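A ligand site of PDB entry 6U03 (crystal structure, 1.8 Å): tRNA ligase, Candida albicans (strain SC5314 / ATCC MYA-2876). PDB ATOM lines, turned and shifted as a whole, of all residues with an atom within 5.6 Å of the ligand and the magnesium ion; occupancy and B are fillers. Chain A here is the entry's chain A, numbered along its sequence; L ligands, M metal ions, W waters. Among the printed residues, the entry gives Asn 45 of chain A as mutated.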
ATOM      1  N   THR A  20      19.686  15.509  14.544  1.00  0.00           N
ATOM      2  CA  THR A  20      18.448  15.049  13.933  1.00  0.00           C
ATOM      3  C   THR A  20      18.792  14.139  12.758  1.00  0.00           C
ATOM      4  O   THR A  20      19.952  13.888  12.455  1.00  0.00           O
ATOM      5  CB  THR A  20      17.580  16.235  13.479  1.00  0.00           C
ATOM      6  OG1 THR A  20      18.329  17.072  12.593  1.00  0.00           O
ATOM      7  CG2 THR A  20      17.135  17.048  14.703  1.00  0.00           C
ATOM      8  N   ILE A  21      17.759  13.608  12.093  1.00  0.00           N
ATOM      9  CA  ILE A  21      17.994  12.655  11.025  1.00  0.00           C
ATOM     10  C   ILE A  21      18.801  13.313   9.905  1.00  0.00           C
ATOM     11  O   ILE A  21      18.536  14.464   9.507  1.00  0.00           O
ATOM     12  CB  ILE A  21      16.661  12.105  10.505  1.00  0.00           C
ATOM     13  CG1 ILE A  21      15.992  11.274  11.608  1.00  0.00           C
ATOM     14  CG2 ILE A  21      16.851  11.322   9.223  1.00  0.00           C
ATOM     15  CD1 ILE A  21      14.609  10.698  11.213  1.00  0.00           C
ATOM     16  N   GLY A  22      19.799  12.576   9.416  1.00  0.00           N
ATOM     17  CA  GLY A  22      20.585  13.004   8.283  1.00  0.00           C
ATOM     18  C   GLY A  22      21.661  14.027   8.574  1.00  0.00           C
ATOM     19  O   GLY A  22      22.226  14.576   7.634  1.00  0.00           O
ATOM     20  N   CYS A  23      21.957  14.297   9.855  1.00  0.00           N
ATOM     21  CA  CYS A  23      23.054  15.178  10.219  1.00  0.00           C
ATOM     22  C   CYS A  23      24.418  14.555   9.930  1.00  0.00           C
ATOM     23  O   CYS A  23      25.423  15.258  10.046  1.00  0.00           O
ATOM     24  CB  CYS A  23      22.944  15.593  11.708  1.00  0.00           C
ATOM     25  SG  CYS A  23      21.679  16.807  12.015  1.00  0.00           S
ATOM     26  N   GLY A  24      24.483  13.267   9.621  1.00  0.00           N
ATOM     27  CA  GLY A  24      25.737  12.591   9.372  1.00  0.00           C
ATOM     28  C   GLY A  24      26.257  11.774  10.513  1.00  0.00           C
ATOM     29  O   GLY A  24      27.441  11.448  10.511  1.00  0.00           O
ATOM     30  N   LYS A  25      25.411  11.447  11.513  1.00  0.00           N
ATOM     31  CA  LYS A  25      25.848  10.669  12.662  1.00  0.00           C
ATOM     32  C   LYS A  25      26.545   9.386  12.227  1.00  0.00           C
ATOM     33  O   LYS A  25      27.675   9.087  12.643  1.00  0.00           O
ATOM     34  CB  LYS A  25      24.669  10.303  13.564  1.00  0.00           C
ATOM     35  CG  LYS A  25      23.954  11.439  14.248  1.00  0.00           C
ATOM     36  CD  LYS A  25      22.871  10.875  15.176  1.00  0.00           C
ATOM     37  CE  LYS A  25      21.831  10.048  14.397  1.00  0.00           C
ATOM     38  NZ  LYS A  25      21.140  10.891  13.354  1.00  0.00           N
ATOM     39  N   THR A  26      25.863   8.603  11.389  1.00  0.00           N
ATOM     40  CA  THR A  26      26.365   7.291  11.042  1.00  0.00           C
ATOM     41  C   THR A  26      27.601   7.386  10.160  1.00  0.00           C
ATOM     42  O   THR A  26      28.521   6.566  10.292  1.00  0.00           O
ATOM     43  CB  THR A  26      25.252   6.485  10.381  1.00  0.00           C
ATOM     44  OG1 THR A  26      24.191   6.363  11.330  1.00  0.00           O
ATOM     45  CG2 THR A  26      25.727   5.104   9.974  1.00  0.00           C
ATOM     46  N   THR A  27      27.641   8.380   9.267  1.00  0.00           N
ATOM     47  CA  THR A  27      28.806   8.570   8.422  1.00  0.00           C
ATOM     48  C   THR A  27      30.029   8.948   9.254  1.00  0.00           C
ATOM     49  O   THR A  27      31.135   8.433   9.038  1.00  0.00           O
ATOM     50  CB  THR A  27      28.527   9.657   7.378  1.00  0.00           C
ATOM     51  OG1 THR A  27      27.368   9.272   6.613  1.00  0.00           O
ATOM     52  CG2 THR A  27      29.715   9.826   6.434  1.00  0.00           C
ATOM     53  N   VAL A  28      29.840   9.870  10.191  1.00  0.00           N
ATOM     54  CA  VAL A  28      30.948  10.273  11.078  1.00  0.00           C
ATOM     55  C   VAL A  28      31.390   9.095  11.936  1.00  0.00           C
ATOM     56  O   VAL A  28      32.582   8.803  12.076  1.00  0.00           O
ATOM     57  CB  VAL A  28      30.515  11.482  11.927  1.00  0.00           C
ATOM     58  CG1 VAL A  28      31.522  11.735  13.059  1.00  0.00           C
ATOM     59  CG2 VAL A  28      30.375  12.732  11.033  1.00  0.00           C
ATOM     60  N   GLN A  43      24.247   1.085  16.700  1.00  0.00           N
ATOM     61  CA  GLN A  43      23.296   1.861  15.909  1.00  0.00           C
ATOM     62  C   GLN A  43      21.875   1.584  16.416  1.00  0.00           C
ATOM     63  O   GLN A  43      21.376   0.463  16.292  1.00  0.00           O
ATOM     64  CB  GLN A  43      23.455   1.528  14.429  1.00  0.00           C
ATOM     65  CG  GLN A  43      24.732   2.142  13.846  1.00  0.00           C
ATOM     66  CD  GLN A  43      24.945   1.788  12.378  1.00  0.00           C
ATOM     67  OE1 GLN A  43      25.841   1.016  12.038  1.00  0.00           O
ATOM     68  NE2 GLN A  43      24.102   2.337  11.514  1.00  0.00           N
ATOM     69  N   ASN A  45      19.162   2.411  15.173  1.00  0.00           N
ATOM     70  CA  ASN A  45      18.287   2.006  14.063  1.00  0.00           C
ATOM     71  C   ASN A  45      18.319   0.499  13.826  1.00  0.00           C
ATOM     72  O   ASN A  45      17.328  -0.069  13.364  1.00  0.00           O
ATOM     73  CB  ASN A  45      18.693   2.755  12.787  1.00  0.00           C
ATOM     74  CG  ASN A  45      18.115   4.163  12.731  1.00  0.00           C
ATOM     75  OD1 ASN A  45      17.029   4.406  13.243  1.00  0.00           O
ATOM     76  ND2 ASN A  45      18.843   5.081  12.090  1.00  0.00           N
ATOM     77  N   ASP A  74      25.000   5.657  18.667  1.00  0.00           N
ATOM     78  CA  ASP A  74      24.466   6.246  17.432  1.00  0.00           C
ATOM     79  C   ASP A  74      22.942   6.342  17.523  1.00  0.00           C
ATOM     80  O   ASP A  74      22.207   5.447  17.100  1.00  0.00           O
ATOM     81  CB  ASP A  74      24.941   5.450  16.235  1.00  0.00           C
ATOM     82  CG  ASP A  74      24.676   6.137  14.905  1.00  0.00           C
ATOM     83  OD1 ASP A  74      23.826   7.037  14.857  1.00  0.00           O
ATOM     84  OD2 ASP A  74      25.332   5.769  13.905  1.00  0.00           O
ATOM     85  N   ASN A  76      19.810   9.863  17.737  1.00  0.00           N
ATOM     86  CA  ASN A  76      19.690  11.319  17.567  1.00  0.00           C
ATOM     87  C   ASN A  76      19.831  12.077  18.889  1.00  0.00           C
ATOM     88  O   ASN A  76      20.589  13.041  18.977  1.00  0.00           O
ATOM     89  CB  ASN A  76      18.359  11.660  16.893  1.00  0.00           C
ATOM     90  CG  ASN A  76      18.411  11.436  15.412  1.00  0.00           C
ATOM     91  OD1 ASN A  76      19.314  11.926  14.746  1.00  0.00           O
ATOM     92  ND2 ASN A  76      17.466  10.654  14.893  1.00  0.00           N
ATOM     93  N   ARG A 128      19.931  15.767   1.879  1.00  0.00           N
ATOM     94  CA  ARG A 128      20.792  14.592   2.029  1.00  0.00           C
ATOM     95  C   ARG A 128      19.974  13.317   2.044  1.00  0.00           C
ATOM     96  O   ARG A 128      20.364  12.306   1.455  1.00  0.00           O
ATOM     97  CB  ARG A 128      21.586  14.696   3.320  1.00  0.00           C
ATOM     98  CG  ARG A 128      22.734  15.677   3.290  1.00  0.00           C
ATOM     99  CD  ARG A 128      23.462  15.584   4.612  1.00  0.00           C
ATOM    100  NE  ARG A 128      24.559  16.538   4.707  1.00  0.00           N
ATOM    101  CZ  ARG A 128      25.243  16.782   5.827  1.00  0.00           C
ATOM    102  NH1 ARG A 128      24.930  16.136   6.943  1.00  0.00           N
ATOM    103  NH2 ARG A 128      26.228  17.663   5.830  1.00  0.00           N
ATOM    104  N   VAL A 129      18.832  13.339   2.728  1.00  0.00           N
ATOM    105  CA  VAL A 129      18.067  12.112   2.938  1.00  0.00           C
ATOM    106  C   VAL A 129      17.296  11.742   1.679  1.00  0.00           C
ATOM    107  O   VAL A 129      17.227  10.559   1.322  1.00  0.00           O
ATOM    108  CB  VAL A 129      17.150  12.277   4.171  1.00  0.00           C
ATOM    109  CG1 VAL A 129      16.132  11.131   4.244  1.00  0.00           C
ATOM    110  CG2 VAL A 129      17.978  12.322   5.457  1.00  0.00           C
ATOM    111  N   ARG A 132      19.496   9.993  -0.916  1.00  0.00           N
ATOM    112  CA  ARG A 132      19.809   8.588  -0.678  1.00  0.00           C
ATOM    113  C   ARG A 132      18.541   7.742  -0.720  1.00  0.00           C
ATOM    114  O   ARG A 132      17.720   7.856  -1.636  1.00  0.00           O
ATOM    115  CB  ARG A 132      20.527   8.416   0.665  1.00  0.00           C
ATOM    116  CG  ARG A 132      19.700   8.827   1.865  1.00  0.00           C
ATOM    117  CD  ARG A 132      20.133   8.140   3.149  1.00  0.00           C
ATOM    118  NE  ARG A 132      19.023   8.053   4.094  1.00  0.00           N
ATOM    119  CZ  ARG A 132      19.168   7.909   5.408  1.00  0.00           C
ATOM    120  NH1 ARG A 132      20.376   7.847   5.948  1.00  0.00           N
ATOM    121  NH2 ARG A 132      18.097   7.846   6.192  1.00  0.00           N
ATOM    122  N   ASP A 183      28.197  21.456   1.482  1.00  0.00           N
ATOM    123  CA  ASP A 183      29.603  21.241   1.226  1.00  0.00           C
ATOM    124  C   ASP A 183      30.157  22.422   0.437  1.00  0.00           C
ATOM    125  O   ASP A 183      29.457  23.036  -0.379  1.00  0.00           O
ATOM    126  CB  ASP A 183      29.832  19.923   0.484  1.00  0.00           C
ATOM    127  CG  ASP A 183      29.083  18.748   1.132  1.00  0.00           C
ATOM    128  OD1 ASP A 183      29.039  18.657   2.379  1.00  0.00           O
ATOM    129  OD2 ASP A 183      28.544  17.922   0.377  1.00  0.00           O
ATOM    130  N   LYS A 188      33.314  17.662   2.208  1.00  0.00           N
ATOM    131  CA  LYS A 188      32.071  17.317   2.886  1.00  0.00           C
ATOM    132  C   LYS A 188      32.131  17.761   4.340  1.00  0.00           C
ATOM    133  O   LYS A 188      33.179  17.658   4.988  1.00  0.00           O
ATOM    134  CB  LYS A 188      31.813  15.811   2.815  1.00  0.00           C
ATOM    135  CG  LYS A 188      31.896  15.218   1.418  1.00  0.00           C
ATOM    136  CD  LYS A 188      30.545  14.776   0.894  1.00  0.00           C
ATOM    137  CE  LYS A 188      30.594  14.550  -0.617  1.00  0.00           C
ATOM    138  NZ  LYS A 188      30.892  15.792  -1.400  1.00  0.00           N
ATOM    139  N   SER A 189      31.018  18.269   4.860  1.00  0.00           N
ATOM    140  CA  SER A 189      31.071  18.733   6.236  1.00  0.00           C
ATOM    141  C   SER A 189      31.314  17.581   7.198  1.00  0.00           C
ATOM    142  O   SER A 189      31.981  17.773   8.227  1.00  0.00           O
ATOM    143  CB  SER A 189      29.817  19.537   6.626  1.00  0.00           C
ATOM    144  OG  SER A 189      28.639  18.776   6.621  1.00  0.00           O
ATOM    145  N   SER A 190      30.851  16.365   6.880  1.00  0.00           N
ATOM    146  CA  SER A 190      31.104  15.234   7.776  1.00  0.00           C
ATOM    147  C   SER A 190      32.584  14.886   7.846  1.00  0.00           C
ATOM    148  O   SER A 190      33.065  14.437   8.896  1.00  0.00           O
ATOM    149  CB  SER A 190      30.300  14.001   7.352  1.00  0.00           C
ATOM    150  OG  SER A 190      28.915  14.193   7.598  1.00  0.00           O
ATOM    151  N   LEU A 191      33.330  15.064   6.744  1.00  0.00           N
ATOM    152  CA  LEU A 191      34.779  14.863   6.771  1.00  0.00           C
ATOM    153  C   LEU A 191      35.452  15.917   7.642  1.00  0.00           C
ATOM    154  O   LEU A 191      36.342  15.603   8.449  1.00  0.00           O
ATOM    155  CB  LEU A 191      35.362  14.890   5.347  1.00  0.00           C
ATOM    156  CG  LEU A 191      36.907  14.817   5.242  1.00  0.00           C
ATOM    157  CD1 LEU A 191      37.481  13.599   5.956  1.00  0.00           C
ATOM    158  CD2 LEU A 191      37.392  14.852   3.781  1.00  0.00           C
ATOM    159  N   PHE A 222      36.973   7.940   5.426  1.00  0.00           N
ATOM    160  CA  PHE A 222      35.743   8.676   5.187  1.00  0.00           C
ATOM    161  C   PHE A 222      35.096   8.273   3.861  1.00  0.00           C
ATOM    162  O   PHE A 222      33.879   8.037   3.800  1.00  0.00           O
ATOM    163  CB  PHE A 222      36.027  10.184   5.205  1.00  0.00           C
ATOM    164  CG  PHE A 222      34.844  10.999   4.873  1.00  0.00           C
ATOM    165  CD1 PHE A 222      33.806  11.145   5.795  1.00  0.00           C
ATOM    166  CD2 PHE A 222      34.716  11.606   3.620  1.00  0.00           C
ATOM    167  CE1 PHE A 222      32.673  11.882   5.471  1.00  0.00           C
ATOM    168  CE2 PHE A 222      33.589  12.335   3.306  1.00  0.00           C
ATOM    169  CZ  PHE A 222      32.570  12.469   4.236  1.00  0.00           C
ATOM    170  N   ALA A 225      33.103   5.229   4.342  1.00  0.00           N
ATOM    171  CA  ALA A 225      31.838   5.499   5.016  1.00  0.00           C
ATOM    172  C   ALA A 225      30.864   6.214   4.091  1.00  0.00           C
ATOM    173  O   ALA A 225      29.660   5.911   4.089  1.00  0.00           O
ATOM    174  CB  ALA A 225      32.075   6.318   6.283  1.00  0.00           C
ATOM    175  N   LEU A 226      31.369   7.170   3.309  1.00  0.00           N
ATOM    176  CA  LEU A 226      30.497   7.993   2.472  1.00  0.00           C
ATOM    177  C   LEU A 226      29.844   7.152   1.394  1.00  0.00           C
ATOM    178  O   LEU A 226      28.633   7.266   1.163  1.00  0.00           O
ATOM    179  CB  LEU A 226      31.313   9.140   1.853  1.00  0.00           C
ATOM    180  CG  LEU A 226      30.549  10.250   1.142  1.00  0.00           C
ATOM    181  CD1 LEU A 226      29.675  10.993   2.128  1.00  0.00           C
ATOM    182  CD2 LEU A 226      31.518  11.196   0.435  1.00  0.00           C
HETATM  183  P1  LIG L   1      19.847   8.673  10.153  1.00  0.00           P
HETATM  184  O1  LIG L   1      20.546   7.338  10.307  1.00  0.00           O
HETATM  185  O2  LIG L   1      18.710   8.532   9.175  1.00  0.00           O
HETATM  186  O3  LIG L   1      19.331   9.105  11.520  1.00  0.00           O
HETATM  187  O4  LIG L   1      20.812   9.846   9.600  1.00  0.00           O
HETATM  188  P2  LIG L   1      22.353  10.031   9.989  1.00  0.00           P
HETATM  189  O5  LIG L   1      22.990   8.773  10.446  1.00  0.00           O
HETATM  190  O6  LIG L   1      22.510  11.189  10.967  1.00  0.00           O
HETATM  191  O7  LIG L   1      23.077  10.584   8.634  1.00  0.00           O
HETATM  192  P3  LIG L   1      23.921   9.707   7.618  1.00  0.00           P
HETATM  193  O8  LIG L   1      25.347   9.525   8.107  1.00  0.00           O
HETATM  194  O9  LIG L   1      23.255   8.384   7.321  1.00  0.00           O
HETATM  195  O10 LIG L   1      23.930  10.641   6.310  1.00  0.00           O
HETATM  196  C1  LIG L   1      22.733  10.840   5.566  1.00  0.00           C
HETATM  197  C2  LIG L   1      23.105  10.898   4.087  1.00  0.00           C
HETATM  198  O11 LIG L   1      23.915  12.048   3.909  1.00  0.00           O
HETATM  199  C3  LIG L   1      23.908   9.711   3.579  1.00  0.00           C
HETATM  200  O12 LIG L   1      23.479   9.482   2.238  1.00  0.00           O
HETATM  201  C4  LIG L   1      25.346  10.232   3.592  1.00  0.00           C
HETATM  202  O13 LIG L   1      26.172   9.611   2.642  1.00  0.00           O
HETATM  203  C5  LIG L   1      25.151  11.713   3.318  1.00  0.00           C
HETATM  204  N1  LIG L   1      26.137  12.591   3.960  1.00  0.00           N
HETATM  205  C6  LIG L   1      26.726  12.461   5.202  1.00  0.00           C
HETATM  206  N2  LIG L   1      27.570  13.506   5.385  1.00  0.00           N
HETATM  207  C7  LIG L   1      27.514  14.297   4.287  1.00  0.00           C
HETATM  208  C8  LIG L   1      28.156  15.479   3.942  1.00  0.00           C
HETATM  209  O14 LIG L   1      28.967  16.031   4.710  1.00  0.00           O
HETATM  210  N3  LIG L   1      27.883  16.044   2.708  1.00  0.00           N
HETATM  211  C9  LIG L   1      26.998  15.473   1.838  1.00  0.00           C
HETATM  212  N4  LIG L   1      26.747  16.047   0.658  1.00  0.00           N
HETATM  213  N5  LIG L   1      26.363  14.314   2.187  1.00  0.00           N
HETATM  214  C10 LIG L   1      26.623  13.738   3.390  1.00  0.00           C
HETATM  215 MG    MG M   1      22.315   6.887  10.933  1.00  0.00          MG
HETATM  216  O   HOH W   1      26.807  12.622  -0.455  1.00  0.00           O
HETATM  217  O   HOH W   2      24.199   7.338   1.057  1.00  0.00           O
HETATM  218  O   HOH W   3      27.298   7.734   4.089  1.00  0.00           O
HETATM  219  O   HOH W   4      22.031   7.069  12.917  1.00  0.00           O
HETATM  220  O   HOH W   5      22.545   6.349   8.755  1.00  0.00           O
HETATM  221  O   HOH W   6      22.883  11.677   0.496  1.00  0.00           O
HETATM  222  O   HOH W   7      25.612   6.336   6.404  1.00  0.00           O
HETATM  223  O   HOH W   8      22.537   6.489   4.623  1.00  0.00           O
HETATM  224  O   HOH W   9      26.769   9.962  -0.203  1.00  0.00           O
HETATM  225  O   HOH W  10      16.442   7.430   8.993  1.00  0.00           O
HETATM  226  O   HOH W  11      21.540   4.579  11.091  1.00  0.00           O
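O14 of the ligand lies within hydrogen-bond range of N of Ser 190 (2.9 Å). N of Cys 23 is in hydrogen-bond range of O6 of the ligand (3.3 Å). An oxygen (O8) of the ligand is in hydrogen-bond range of the backbone NH of Thr 27 (2.8 Å). N of Lys 25 is in hydrogen-bond range of O6 of the ligand (3.0 Å). NZ of Lys 25 lies within salt-bridge range of O6 of the ligand. OG of Ser 190 is in hydrogen-bond range of N2 of the ligand, at 2.7 Å. The backbone NH (N) of Gly 24 sits at hydrogen-bond distance from an oxygen (O6) of the ligand, 3.2 Å away. O8 of the ligand sits at hydrogen-bond distance from OG1 of Thr 27 (2.5 Å). NH2 of Arg 128 sits at hydrogen-bond distance from O14 of the ligand (3.4 Å). The backbone NH (N) of Gly 22 is in hydrogen-bond range of an oxygen (O4) of the ligand (2.9 Å). The guanidinium group (NH2) of Arg 132 is in salt-bridge range of an oxygen (O2) of the ligand. The side-chain hydroxyl (OG) of Ser 189 sits at hydrogen-bond distance from an oxygen (O14) of the ligand (3.4 Å). O1 of the ligand lies close to ND2 of Asn 45 (3.3 Å). A nitrogen (N4) of the ligand lies within hydrogen-bond range of the side-chain carboxylate of Asp 183. O14 of the ligand lies within hydrogen-bond range of N of Ser 189 (3.0 Å). The backbone NH (N) of Thr 26 lies within hydrogen-bond range of an oxygen (O8) of the ligand.
O of Cys 23 is in hydrogen-bond range of NH1 of Arg 128 (3.3 Å). The side-chain amino group (NZ) of Lys 25 sits at hydrogen-bond distance from the side-chain amide oxygen (OD1) of Asn 76 (2.5 Å). OG1 of Thr 26 lies close to OD2 of Asp 74. OD1 of Asp 183 sits at hydrogen-bond distance from N of Ser 189 (3.2 Å). The side-chain carboxylate (OD2) of Asp 183 lies within salt-bridge range of the side-chain amino group (NZ) of Lys 188 (3.6 Å). The side-chain hydroxyl (OG1) of Thr 20 lies within hydrogen-bond range of the side-chain sulfur (SG) of Cys 23 (3.4 Å). The backbone carbonyl oxygen of Thr 20 lies within hydrogen-bond range of the side-chain amino group of Lys 25. O of Gly 22 sits at hydrogen-bond distance from NH1 of Arg 128 (3.2 Å).
Ile 21 touches the ligand (CG2 to O2, 3.4 Å). Lys 188 touches the ligand (CB to O14, 3.4 Å). Leu 226 touches the ligand. Hydrophobic or aromatic side chains that line the ligand: Ile 21 and Leu 226. Within 4 Å of the ligand: Ile 21, Gly 22, Cys 23, Gly 24, Lys 25, Thr 26, Thr 27, Asn 45, Arg 128, Arg 132, Asp 183, Lys 188, Ser 189, Ser 190 and Leu 226. The nearest printed residue that does not touch the ligand is Thr 20 (4.01 Å).
One residue has an atom within 4 Å of the magnesium ion: Thr 26.
The magnesium ion is bound by an oxygen (O1) of the ligand, the side-chain hydroxyl (OG1) of Thr 26, water W4, an oxygen (O5) of the ligand, water W5 and water W11.
Water W11 bridges the side-chain amide nitrogen (ND2) of Asn 45 (2.9 Å) and the side-chain amide nitrogen (NE2) of Gln 43 (3.4 Å). Water W10 lies within hydrogen-bond range of O2 of the ligand and NH2 of Arg 132. Water W3 lies within hydrogen-bond range of O13 of the ligand (2.6 Å), OG1 of Thr 27 (3.0 Å), O of Ala 225 (3.0 Å) and O of Leu 226 (3.3 Å). Water W6 bridges the backbone carbonyl oxygen (O) of Arg 128 (2.8 Å) and an oxygen (O12) of the ligand (2.9 Å). Water W7 lies within hydrogen-bond range of an oxygen (O9) of the ligand and the side-chain hydroxyl (OG1) of Thr 27. Water W8 bridges the guanidinium group of Arg 132 (2.9 Å) and an oxygen (O9) of the ligand (3.4 Å).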
